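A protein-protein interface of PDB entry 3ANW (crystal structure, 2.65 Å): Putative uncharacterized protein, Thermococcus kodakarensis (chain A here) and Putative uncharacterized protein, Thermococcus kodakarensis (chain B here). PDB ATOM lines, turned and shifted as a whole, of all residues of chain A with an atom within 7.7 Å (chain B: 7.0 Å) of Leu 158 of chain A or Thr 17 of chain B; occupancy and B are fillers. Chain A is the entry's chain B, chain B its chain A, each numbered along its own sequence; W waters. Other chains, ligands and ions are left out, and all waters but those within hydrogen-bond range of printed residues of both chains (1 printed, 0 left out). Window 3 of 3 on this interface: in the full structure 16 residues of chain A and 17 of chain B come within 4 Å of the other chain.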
ATOM      1  N   ILE A 132      35.257  20.544 -21.910  1.00  0.00           N
ATOM      2  CA  ILE A 132      34.131  20.037 -21.124  1.00  0.00           C
ATOM      3  C   ILE A 132      34.235  20.637 -19.727  1.00  0.00           C
ATOM      4  O   ILE A 132      33.254  21.148 -19.191  1.00  0.00           O
ATOM      5  CB  ILE A 132      34.118  18.477 -21.050  1.00  0.00           C
ATOM      6  CG1 ILE A 132      33.769  17.870 -22.412  1.00  0.00           C
ATOM      7  CG2 ILE A 132      33.093  17.996 -20.051  1.00  0.00           C
ATOM      8  CD1 ILE A 132      34.142  16.395 -22.546  1.00  0.00           C
ATOM      9  N   VAL A 136      31.273  23.065 -17.948  1.00  0.00           N
ATOM     10  CA  VAL A 136      30.631  22.754 -16.681  1.00  0.00           C
ATOM     11  C   VAL A 136      30.502  24.074 -15.910  1.00  0.00           C
ATOM     12  O   VAL A 136      29.536  24.303 -15.182  1.00  0.00           O
ATOM     13  CB  VAL A 136      31.509  21.737 -15.885  1.00  0.00           C
ATOM     14  CG1 VAL A 136      31.053  21.621 -14.433  1.00  0.00           C
ATOM     15  CG2 VAL A 136      31.487  20.371 -16.568  1.00  0.00           C
ATOM     16  N   ASN A 141      24.617  21.870 -16.335  1.00  0.00           N
ATOM     17  CA  ASN A 141      24.087  20.962 -17.355  1.00  0.00           C
ATOM     18  C   ASN A 141      23.402  21.714 -18.500  1.00  0.00           C
ATOM     19  O   ASN A 141      23.007  22.880 -18.349  1.00  0.00           O
ATOM     20  CB  ASN A 141      23.095  19.943 -16.754  1.00  0.00           C
ATOM     21  CG  ASN A 141      23.664  19.203 -15.540  1.00  0.00           C
ATOM     22  OD1 ASN A 141      24.326  18.166 -15.677  1.00  0.00           O
ATOM     23  ND2 ASN A 141      23.385  19.729 -14.341  1.00  0.00           N
ATOM     24  N   SER A 142      23.285  21.028 -19.639  1.00  0.00           N
ATOM     25  CA  SER A 142      22.659  21.555 -20.859  1.00  0.00           C
ATOM     26  C   SER A 142      22.505  20.411 -21.872  1.00  0.00           C
ATOM     27  O   SER A 142      23.491  19.799 -22.293  1.00  0.00           O
ATOM     28  CB  SER A 142      23.502  22.691 -21.465  1.00  0.00           C
ATOM     29  OG  SER A 142      23.067  23.012 -22.783  1.00  0.00           O
ATOM     30  N   LEU A 146      25.166  17.642 -24.905  1.00  0.00           N
ATOM     31  CA  LEU A 146      25.240  16.191 -24.887  1.00  0.00           C
ATOM     32  C   LEU A 146      25.121  15.637 -26.286  1.00  0.00           C
ATOM     33  O   LEU A 146      25.816  14.688 -26.639  1.00  0.00           O
ATOM     34  CB  LEU A 146      24.150  15.597 -24.007  1.00  0.00           C
ATOM     35  CG  LEU A 146      24.239  15.836 -22.501  1.00  0.00           C
ATOM     36  CD1 LEU A 146      23.215  14.951 -21.810  1.00  0.00           C
ATOM     37  CD2 LEU A 146      25.636  15.529 -21.986  1.00  0.00           C
ATOM     38  N   LEU A 149      28.624  15.232 -27.678  1.00  0.00           N
ATOM     39  CA  LEU A 149      29.675  14.458 -27.035  1.00  0.00           C
ATOM     40  C   LEU A 149      29.552  12.957 -27.268  1.00  0.00           C
ATOM     41  O   LEU A 149      28.454  12.441 -27.467  1.00  0.00           O
ATOM     42  CB  LEU A 149      29.659  14.723 -25.528  1.00  0.00           C
ATOM     43  CG  LEU A 149      29.822  16.164 -25.067  1.00  0.00           C
ATOM     44  CD1 LEU A 149      29.625  16.222 -23.584  1.00  0.00           C
ATOM     45  CD2 LEU A 149      31.194  16.684 -25.442  1.00  0.00           C
ATOM     46  N   PRO A 151      29.359   9.211 -26.042  1.00  0.00           N
ATOM     47  CA  PRO A 151      28.739   8.669 -24.821  1.00  0.00           C
ATOM     48  C   PRO A 151      29.605   8.625 -23.556  1.00  0.00           C
ATOM     49  O   PRO A 151      29.103   8.832 -22.463  1.00  0.00           O
ATOM     50  CB  PRO A 151      28.301   7.278 -25.264  1.00  0.00           C
ATOM     51  CG  PRO A 151      27.912   7.515 -26.668  1.00  0.00           C
ATOM     52  CD  PRO A 151      29.030   8.362 -27.198  1.00  0.00           C
ATOM     53  N   GLU A 152      30.900   8.380 -23.701  1.00  0.00           N
ATOM     54  CA  GLU A 152      31.807   8.338 -22.552  1.00  0.00           C
ATOM     55  C   GLU A 152      32.093   9.748 -22.021  1.00  0.00           C
ATOM     56  O   GLU A 152      32.283   9.918 -20.823  1.00  0.00           O
ATOM     57  CB  GLU A 152      33.125   7.635 -22.907  1.00  0.00           C
ATOM     58  CG  GLU A 152      32.993   6.385 -23.795  1.00  0.00           C
ATOM     59  CD  GLU A 152      32.944   6.699 -25.303  1.00  0.00           C
ATOM     60  OE1 GLU A 152      33.321   5.831 -26.118  1.00  0.00           O
ATOM     61  OE2 GLU A 152      32.543   7.811 -25.689  1.00  0.00           O
ATOM     62  N   GLU A 153      32.142  10.741 -22.914  1.00  0.00           N
ATOM     63  CA  GLU A 153      32.379  12.139 -22.546  1.00  0.00           C
ATOM     64  C   GLU A 153      31.109  12.722 -21.945  1.00  0.00           C
ATOM     65  O   GLU A 153      31.150  13.676 -21.180  1.00  0.00           O
ATOM     66  CB  GLU A 153      32.778  12.979 -23.764  1.00  0.00           C
ATOM     67  CG  GLU A 153      34.108  12.619 -24.406  1.00  0.00           C
ATOM     68  CD  GLU A 153      34.450  13.507 -25.592  1.00  0.00           C
ATOM     69  OE1 GLU A 153      35.639  13.904 -25.731  1.00  0.00           O
ATOM     70  OE2 GLU A 153      33.525  13.796 -26.384  1.00  0.00           O
ATOM     71  N   ARG A 154      29.974  12.171 -22.351  1.00  0.00           N
ATOM     72  CA  ARG A 154      28.667  12.580 -21.850  1.00  0.00           C
ATOM     73  C   ARG A 154      28.647  12.272 -20.350  1.00  0.00           C
ATOM     74  O   ARG A 154      28.255  13.106 -19.535  1.00  0.00           O
ATOM     75  CB  ARG A 154      27.582  11.748 -22.532  1.00  0.00           C
ATOM     76  CG  ARG A 154      26.401  12.524 -23.011  1.00  0.00           C
ATOM     77  CD  ARG A 154      26.464  12.700 -24.501  1.00  0.00           C
ATOM     78  NE  ARG A 154      26.301  11.422 -25.176  1.00  0.00           N
ATOM     79  CZ  ARG A 154      25.462  11.201 -26.179  1.00  0.00           C
ATOM     80  NH1 ARG A 154      24.698  12.174 -26.648  1.00  0.00           N
ATOM     81  NH2 ARG A 154      25.368   9.989 -26.697  1.00  0.00           N
ATOM     82  N   ARG A 155      29.046  11.042 -20.021  1.00  0.00           N
ATOM     83  CA  ARG A 155      29.126  10.555 -18.651  1.00  0.00           C
ATOM     84  C   ARG A 155      29.951  11.512 -17.786  1.00  0.00           C
ATOM     85  O   ARG A 155      29.538  11.877 -16.683  1.00  0.00           O
ATOM     86  CB  ARG A 155      29.774   9.167 -18.650  1.00  0.00           C
ATOM     87  CG  ARG A 155      30.155   8.625 -17.273  1.00  0.00           C
ATOM     88  CD  ARG A 155      28.936   8.335 -16.448  1.00  0.00           C
ATOM     89  NE  ARG A 155      29.287   8.023 -15.068  1.00  0.00           N
ATOM     90  CZ  ARG A 155      28.418   8.003 -14.063  1.00  0.00           C
ATOM     91  NH1 ARG A 155      27.137   8.266 -14.286  1.00  0.00           N
ATOM     92  NH2 ARG A 155      28.836   7.770 -12.831  1.00  0.00           N
ATOM     93  N   ILE A 156      31.112  11.901 -18.315  1.00  0.00           N
ATOM     94  CA  ILE A 156      32.057  12.816 -17.675  1.00  0.00           C
ATOM     95  C   ILE A 156      31.446  14.186 -17.395  1.00  0.00           C
ATOM     96  O   ILE A 156      31.572  14.703 -16.293  1.00  0.00           O
ATOM     97  CB  ILE A 156      33.304  12.980 -18.554  1.00  0.00           C
ATOM     98  CG1 ILE A 156      34.105  11.678 -18.553  1.00  0.00           C
ATOM     99  CG2 ILE A 156      34.142  14.146 -18.096  1.00  0.00           C
ATOM    100  CD1 ILE A 156      35.251  11.676 -19.526  1.00  0.00           C
ATOM    101  N   TYR A 157      30.786  14.766 -18.393  1.00  0.00           N
ATOM    102  CA  TYR A 157      30.134  16.069 -18.244  1.00  0.00           C
ATOM    103  C   TYR A 157      29.031  16.002 -17.190  1.00  0.00           C
ATOM    104  O   TYR A 157      28.904  16.893 -16.355  1.00  0.00           O
ATOM    105  CB  TYR A 157      29.563  16.526 -19.584  1.00  0.00           C
ATOM    106  CG  TYR A 157      28.754  17.794 -19.523  1.00  0.00           C
ATOM    107  CD1 TYR A 157      29.329  18.996 -19.122  1.00  0.00           C
ATOM    108  CD2 TYR A 157      27.407  17.795 -19.877  1.00  0.00           C
ATOM    109  CE1 TYR A 157      28.578  20.164 -19.077  1.00  0.00           C
ATOM    110  CE2 TYR A 157      26.651  18.960 -19.839  1.00  0.00           C
ATOM    111  CZ  TYR A 157      27.241  20.137 -19.440  1.00  0.00           C
ATOM    112  OH  TYR A 157      26.493  21.294 -19.432  1.00  0.00           O
ATOM    113  N   LEU A 158      28.242  14.934 -17.227  1.00  0.00           N
ATOM    114  CA  LEU A 158      27.172  14.735 -16.257  1.00  0.00           C
ATOM    115  C   LEU A 158      27.733  14.598 -14.841  1.00  0.00           C
ATOM    116  O   LEU A 158      27.157  15.123 -13.884  1.00  0.00           O
ATOM    117  CB  LEU A 158      26.346  13.509 -16.621  1.00  0.00           C
ATOM    118  CG  LEU A 158      25.456  13.743 -17.841  1.00  0.00           C
ATOM    119  CD1 LEU A 158      24.649  12.505 -18.148  1.00  0.00           C
ATOM    120  CD2 LEU A 158      24.551  14.909 -17.586  1.00  0.00           C
ATOM    121  N   GLN A 159      28.854  13.897 -14.712  1.00  0.00           N
ATOM    122  CA  GLN A 159      29.486  13.727 -13.412  1.00  0.00           C
ATOM    123  C   GLN A 159      30.125  15.030 -12.932  1.00  0.00           C
ATOM    124  O   GLN A 159      29.961  15.401 -11.774  1.00  0.00           O
ATOM    125  CB  GLN A 159      30.534  12.630 -13.452  1.00  0.00           C
ATOM    126  CG  GLN A 159      29.975  11.250 -13.558  1.00  0.00           C
ATOM    127  CD  GLN A 159      31.056  10.194 -13.423  1.00  0.00           C
ATOM    128  OE1 GLN A 159      31.788   9.898 -14.377  1.00  0.00           O
ATOM    129  NE2 GLN A 159      31.180   9.632 -12.223  1.00  0.00           N
ATOM    130  N   MET A 160      30.849  15.713 -13.816  1.00  0.00           N
ATOM    131  CA  MET A 160      31.502  16.975 -13.477  1.00  0.00           C
ATOM    132  C   MET A 160      30.494  17.979 -12.925  1.00  0.00           C
ATOM    133  O   MET A 160      30.751  18.653 -11.935  1.00  0.00           O
ATOM    134  CB  MET A 160      32.123  17.636 -14.721  1.00  0.00           C
ATOM    135  CG  MET A 160      33.240  16.905 -15.431  1.00  0.00           C
ATOM    136  SD  MET A 160      34.743  16.886 -14.498  1.00  0.00           S
ATOM    137  CE  MET A 160      34.933  15.110 -14.250  1.00  0.00           C
ATOM    138  N   SER A 161      29.362  18.096 -13.606  1.00  0.00           N
ATOM    139  CA  SER A 161      28.331  19.046 -13.232  1.00  0.00           C
ATOM    140  C   SER A 161      27.632  18.722 -11.930  1.00  0.00           C
ATOM    141  O   SER A 161      27.226  19.631 -11.208  1.00  0.00           O
ATOM    142  CB  SER A 161      27.321  19.189 -14.363  1.00  0.00           C
ATOM    143  OG  SER A 161      27.990  19.406 -15.591  1.00  0.00           O
ATOM    144  N   LYS A 162      27.471  17.437 -11.634  1.00  0.00           N
ATOM    145  CA  LYS A 162      26.825  17.022 -10.393  1.00  0.00           C
ATOM    146  C   LYS A 162      27.732  17.359  -9.205  1.00  0.00           C
ATOM    147  O   LYS A 162      27.259  17.762  -8.143  1.00  0.00           O
ATOM    148  CB  LYS A 162      26.527  15.523 -10.408  1.00  0.00           C
ATOM    149  CG  LYS A 162      26.003  14.985  -9.082  1.00  0.00           C
ATOM    150  CD  LYS A 162      25.875  13.471  -9.095  1.00  0.00           C
ATOM    151  CE  LYS A 162      25.602  12.926  -7.699  1.00  0.00           C
ATOM    152  NZ  LYS A 162      26.706  13.243  -6.747  1.00  0.00           N
ATOM    153  N   ILE A 163      29.037  17.200  -9.405  1.00  0.00           N
ATOM    154  CA  ILE A 163      30.045  17.476  -8.384  1.00  0.00           C
ATOM    155  C   ILE A 163      30.142  18.982  -8.163  1.00  0.00           C
ATOM    156  O   ILE A 163      30.144  19.476  -7.037  1.00  0.00           O
ATOM    157  CB  ILE A 163      31.402  16.890  -8.834  1.00  0.00           C
ATOM    158  CG1 ILE A 163      31.338  15.362  -8.785  1.00  0.00           C
ATOM    159  CG2 ILE A 163      32.530  17.424  -7.982  1.00  0.00           C
ATOM    160  CD1 ILE A 163      32.458  14.684  -9.497  1.00  0.00           C
ATOM    161  N   ARG A 164      30.167  19.700  -9.268  1.00  0.00           N
ATOM    162  CA  ARG A 164      30.230  21.142  -9.270  1.00  0.00           C
ATOM    163  C   ARG A 164      28.993  21.764  -8.601  1.00  0.00           C
ATOM    164  O   ARG A 164      29.134  22.571  -7.687  1.00  0.00           O
ATOM    165  CB  ARG A 164      30.379  21.615 -10.710  1.00  0.00           C
ATOM    166  CG  ARG A 164      30.569  23.068 -10.868  1.00  0.00           C
ATOM    167  CD  ARG A 164      29.262  23.765 -11.090  1.00  0.00           C
ATOM    168  NE  ARG A 164      29.492  25.117 -11.575  1.00  0.00           N
ATOM    169  CZ  ARG A 164      28.543  26.033 -11.698  1.00  0.00           C
ATOM    170  NH1 ARG A 164      27.294  25.729 -11.368  1.00  0.00           N
ATOM    171  NH2 ARG A 164      28.844  27.251 -12.134  1.00  0.00           N
ATOM    172  N   ALA B  12      23.194   4.355 -23.521  1.00  0.00           N
ATOM    173  CA  ALA B  12      22.050   4.986 -22.866  1.00  0.00           C
ATOM    174  C   ALA B  12      22.188   5.098 -21.352  1.00  0.00           C
ATOM    175  O   ALA B  12      21.488   5.883 -20.713  1.00  0.00           O
ATOM    176  CB  ALA B  12      20.787   4.243 -23.208  1.00  0.00           C
ATOM    177  N   GLU B  13      23.041   4.267 -20.768  1.00  0.00           N
ATOM    178  CA  GLU B  13      23.258   4.326 -19.336  1.00  0.00           C
ATOM    179  C   GLU B  13      24.229   5.459 -19.063  1.00  0.00           C
ATOM    180  O   GLU B  13      24.107   6.162 -18.073  1.00  0.00           O
ATOM    181  CB  GLU B  13      23.834   3.021 -18.815  1.00  0.00           C
ATOM    182  CG  GLU B  13      23.504   2.778 -17.375  1.00  0.00           C
ATOM    183  CD  GLU B  13      22.023   2.679 -17.170  1.00  0.00           C
ATOM    184  OE1 GLU B  13      21.417   3.644 -16.682  1.00  0.00           O
ATOM    185  OE2 GLU B  13      21.449   1.639 -17.526  1.00  0.00           O
ATOM    186  N   LEU B  14      25.170   5.629 -19.985  1.00  0.00           N
ATOM    187  CA  LEU B  14      26.199   6.652 -19.926  1.00  0.00           C
ATOM    188  C   LEU B  14      25.669   8.044 -20.199  1.00  0.00           C
ATOM    189  O   LEU B  14      26.134   9.008 -19.600  1.00  0.00           O
ATOM    190  CB  LEU B  14      27.303   6.336 -20.942  1.00  0.00           C
ATOM    191  CG  LEU B  14      28.279   5.194 -20.639  1.00  0.00           C
ATOM    192  CD1 LEU B  14      29.091   4.811 -21.855  1.00  0.00           C
ATOM    193  CD2 LEU B  14      29.187   5.609 -19.510  1.00  0.00           C
ATOM    194  N   SER B  15      24.670   8.134 -21.073  1.00  0.00           N
ATOM    195  CA  SER B  15      24.085   9.405 -21.494  1.00  0.00           C
ATOM    196  C   SER B  15      23.076  10.107 -20.596  1.00  0.00           C
ATOM    197  O   SER B  15      22.558  11.152 -20.961  1.00  0.00           O
ATOM    198  CB  SER B  15      23.498   9.257 -22.895  1.00  0.00           C
ATOM    199  OG  SER B  15      24.510   9.005 -23.851  1.00  0.00           O
ATOM    200  N   SER B  16      22.807   9.547 -19.427  1.00  0.00           N
ATOM    201  CA  SER B  16      21.860  10.138 -18.487  1.00  0.00           C
ATOM    202  C   SER B  16      22.319   9.785 -17.085  1.00  0.00           C
ATOM    203  O   SER B  16      23.095   8.857 -16.925  1.00  0.00           O
ATOM    204  CB  SER B  16      20.457   9.570 -18.727  1.00  0.00           C
ATOM    205  OG  SER B  16      19.494  10.205 -17.907  1.00  0.00           O
ATOM    206  N   THR B  17      21.908  10.559 -16.082  1.00  0.00           N
ATOM    207  CA  THR B  17      22.272  10.233 -14.707  1.00  0.00           C
ATOM    208  C   THR B  17      21.144   9.408 -14.101  1.00  0.00           C
ATOM    209  O   THR B  17      21.238   8.936 -12.969  1.00  0.00           O
ATOM    210  CB  THR B  17      22.512  11.474 -13.797  1.00  0.00           C
ATOM    211  OG1 THR B  17      21.292  12.191 -13.620  1.00  0.00           O
ATOM    212  CG2 THR B  17      23.574  12.388 -14.360  1.00  0.00           C
ATOM    213  N   ASP B  18      20.073   9.242 -14.865  1.00  0.00           N
ATOM    214  CA  ASP B  18      18.917   8.490 -14.417  1.00  0.00           C
ATOM    215  C   ASP B  18      19.008   7.046 -14.830  1.00  0.00           C
ATOM    216  O   ASP B  18      19.564   6.727 -15.880  1.00  0.00           O
ATOM    217  CB  ASP B  18      17.639   9.063 -15.024  1.00  0.00           C
ATOM    218  CG  ASP B  18      17.410  10.511 -14.663  1.00  0.00           C
ATOM    219  OD1 ASP B  18      17.631  10.900 -13.494  1.00  0.00           O
ATOM    220  OD2 ASP B  18      16.997  11.266 -15.564  1.00  0.00           O
ATOM    221  N   LEU B  19      18.427   6.173 -14.014  1.00  0.00           N
ATOM    222  CA  LEU B  19      18.396   4.759 -14.333  1.00  0.00           C
ATOM    223  C   LEU B  19      17.596   4.582 -15.615  1.00  0.00           C
ATOM    224  O   LEU B  19      16.412   4.903 -15.676  1.00  0.00           O
ATOM    225  CB  LEU B  19      17.713   3.941 -13.235  1.00  0.00           C
ATOM    226  CG  LEU B  19      18.505   3.171 -12.188  1.00  0.00           C
ATOM    227  CD1 LEU B  19      17.553   2.230 -11.467  1.00  0.00           C
ATOM    228  CD2 LEU B  19      19.632   2.390 -12.831  1.00  0.00           C
ATOM    229  N   ASN B  20      18.272   4.106 -16.646  1.00  0.00           N
ATOM    230  CA  ASN B  20      17.649   3.830 -17.928  1.00  0.00           C
ATOM    231  C   ASN B  20      16.558   2.778 -17.660  1.00  0.00           C
ATOM    232  O   ASN B  20      16.775   1.867 -16.877  1.00  0.00           O
ATOM    233  CB  ASN B  20      18.726   3.274 -18.865  1.00  0.00           C
ATOM    234  CG  ASN B  20      18.258   3.124 -20.270  1.00  0.00           C
ATOM    235  OD1 ASN B  20      17.371   3.833 -20.717  1.00  0.00           O
ATOM    236  ND2 ASN B  20      18.865   2.202 -20.990  1.00  0.00           N
ATOM    237  N   LEU B  73      27.387   1.120 -13.774  1.00  0.00           N
ATOM    238  CA  LEU B  73      26.707   2.400 -13.852  1.00  0.00           C
ATOM    239  C   LEU B  73      25.396   2.345 -13.090  1.00  0.00           C
ATOM    240  O   LEU B  73      25.062   3.257 -12.344  1.00  0.00           O
ATOM    241  CB  LEU B  73      26.437   2.787 -15.304  1.00  0.00           C
ATOM    242  CG  LEU B  73      27.634   3.120 -16.185  1.00  0.00           C
ATOM    243  CD1 LEU B  73      27.223   3.166 -17.626  1.00  0.00           C
ATOM    244  CD2 LEU B  73      28.249   4.423 -15.759  1.00  0.00           C
ATOM    245  N   LYS B  77      23.836   4.233  -9.519  1.00  0.00           N
ATOM    246  CA  LYS B  77      22.628   5.014  -9.625  1.00  0.00           C
ATOM    247  C   LYS B  77      21.640   4.472  -8.606  1.00  0.00           C
ATOM    248  O   LYS B  77      20.952   5.247  -7.949  1.00  0.00           O
ATOM    249  CB  LYS B  77      22.049   4.948 -11.033  1.00  0.00           C
ATOM    250  CG  LYS B  77      22.859   5.696 -12.055  1.00  0.00           C
ATOM    251  CD  LYS B  77      22.339   5.465 -13.431  1.00  0.00           C
ATOM    252  CE  LYS B  77      23.225   6.116 -14.440  1.00  0.00           C
ATOM    253  NZ  LYS B  77      22.667   6.004 -15.805  1.00  0.00           N
ATOM    254  N   ASP B  80      22.518   5.636  -5.119  1.00  0.00           N
ATOM    255  CA  ASP B  80      22.080   7.001  -4.928  1.00  0.00           C
ATOM    256  C   ASP B  80      20.577   7.132  -4.694  1.00  0.00           C
ATOM    257  O   ASP B  80      20.143   7.958  -3.903  1.00  0.00           O
ATOM    258  CB  ASP B  80      22.536   7.879  -6.083  1.00  0.00           C
ATOM    259  CG  ASP B  80      23.930   8.442  -5.881  1.00  0.00           C
ATOM    260  OD1 ASP B  80      24.372   8.596  -4.726  1.00  0.00           O
ATOM    261  OD2 ASP B  80      24.586   8.755  -6.893  1.00  0.00           O
HETATM  262  O   HOH W   1      26.345   5.716 -12.355  1.00  0.00           O
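NH2 of Arg 154 of chain A lies within hydrogen-bond range of OG of Ser 15 of chain B, 3.1 Å away.
OG of Ser 16 of chain B sits close to N of Asp 18 of chain B (3.2 Å). The backbone carbonyl oxygen (O) of Ser 16 of chain B lies within hydrogen-bond range of the side-chain amino group (NZ) of Lys 77 of chain B, at 3.1 Å. The backbone carbonyl oxygen (O) of Leu 146 of chain A lies within hydrogen-bond range of the guanidinium group (NH1) of Arg 154 of chain A (2.8 Å). The backbone carbonyl oxygen of Leu 149 of chain A sits at hydrogen-bond distance from the guanidinium group of Arg 154 of chain A, 3.3 Å away. The side-chain amide nitrogen (NE2) of Gln 159 of chain A lies close to the guanidinium group (NH2) of Arg 155 of chain A, at 3.1 Å.
O of Ser 15 of chain B touches CD1 of Leu 146 of chain A (3.9 Å). CB of Leu 14 of chain B touches O of Pro 151 of chain A (3.4 Å). CA of Arg 155 of chain A touches O of Leu 14 of chain B (3.5 Å). Arg 155 of chain A touches Leu 73 of chain B. Leu 158 of chain A touches Ser 15 of chain B (CD1 to O, 3.8 Å). Leu 158 of chain A touches Ser 16 of chain B. Leu 158 of chain A touches Thr 17 of chain B.
Of chain B, only Ser 15, Ser 16 and Thr 17 come within 4 Å of Leu 158 of chain A. Of chain A, only Leu 158 (3.7 Å) comes within 4 Å of Thr 17 of chain B. Of chain A, only Leu 158 (3.7 Å) comes within 4 Å of Ser 16 of chain B. Printed residues of chain A within 4 Å of Leu 14 of chain B: Pro 151 and Arg 155. Of the printed residues of chain B, Leu 146 of chain A touches Ser 15 (3.9 Å). Ile 163 of chain A touches none of the printed residues of chain B. The nearest residue of chain A that does not touch Thr 17 of chain B is Arg 155 of chain A (5.3 Å).
Of the 20 printed residues of chain A, 5 touch a printed residue of chain B. Printed residues of chain A that touch a printed residue of chain B: Leu 146, Pro 151, Arg 154, Arg 155 and Leu 158. Hydrophobic or aromatic side chains of chain A that line the printed part of chain B: Leu 146 and Leu 158. Of the 12 printed residues of chain B, 5 touch a printed residue of chain A. Hydrophobic or aromatic side chains of chain B within 4 Å of the printed part of chain A: Leu 14 and Leu 73. Among the printed residues, no Asp or Glu carboxylate lies within 4 Å of a Lys or Arg side-chain nitrogen of the other chain.
Water W1 bridges O of Leu 73 of chain B and NH2 of Arg 155 of chain A.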
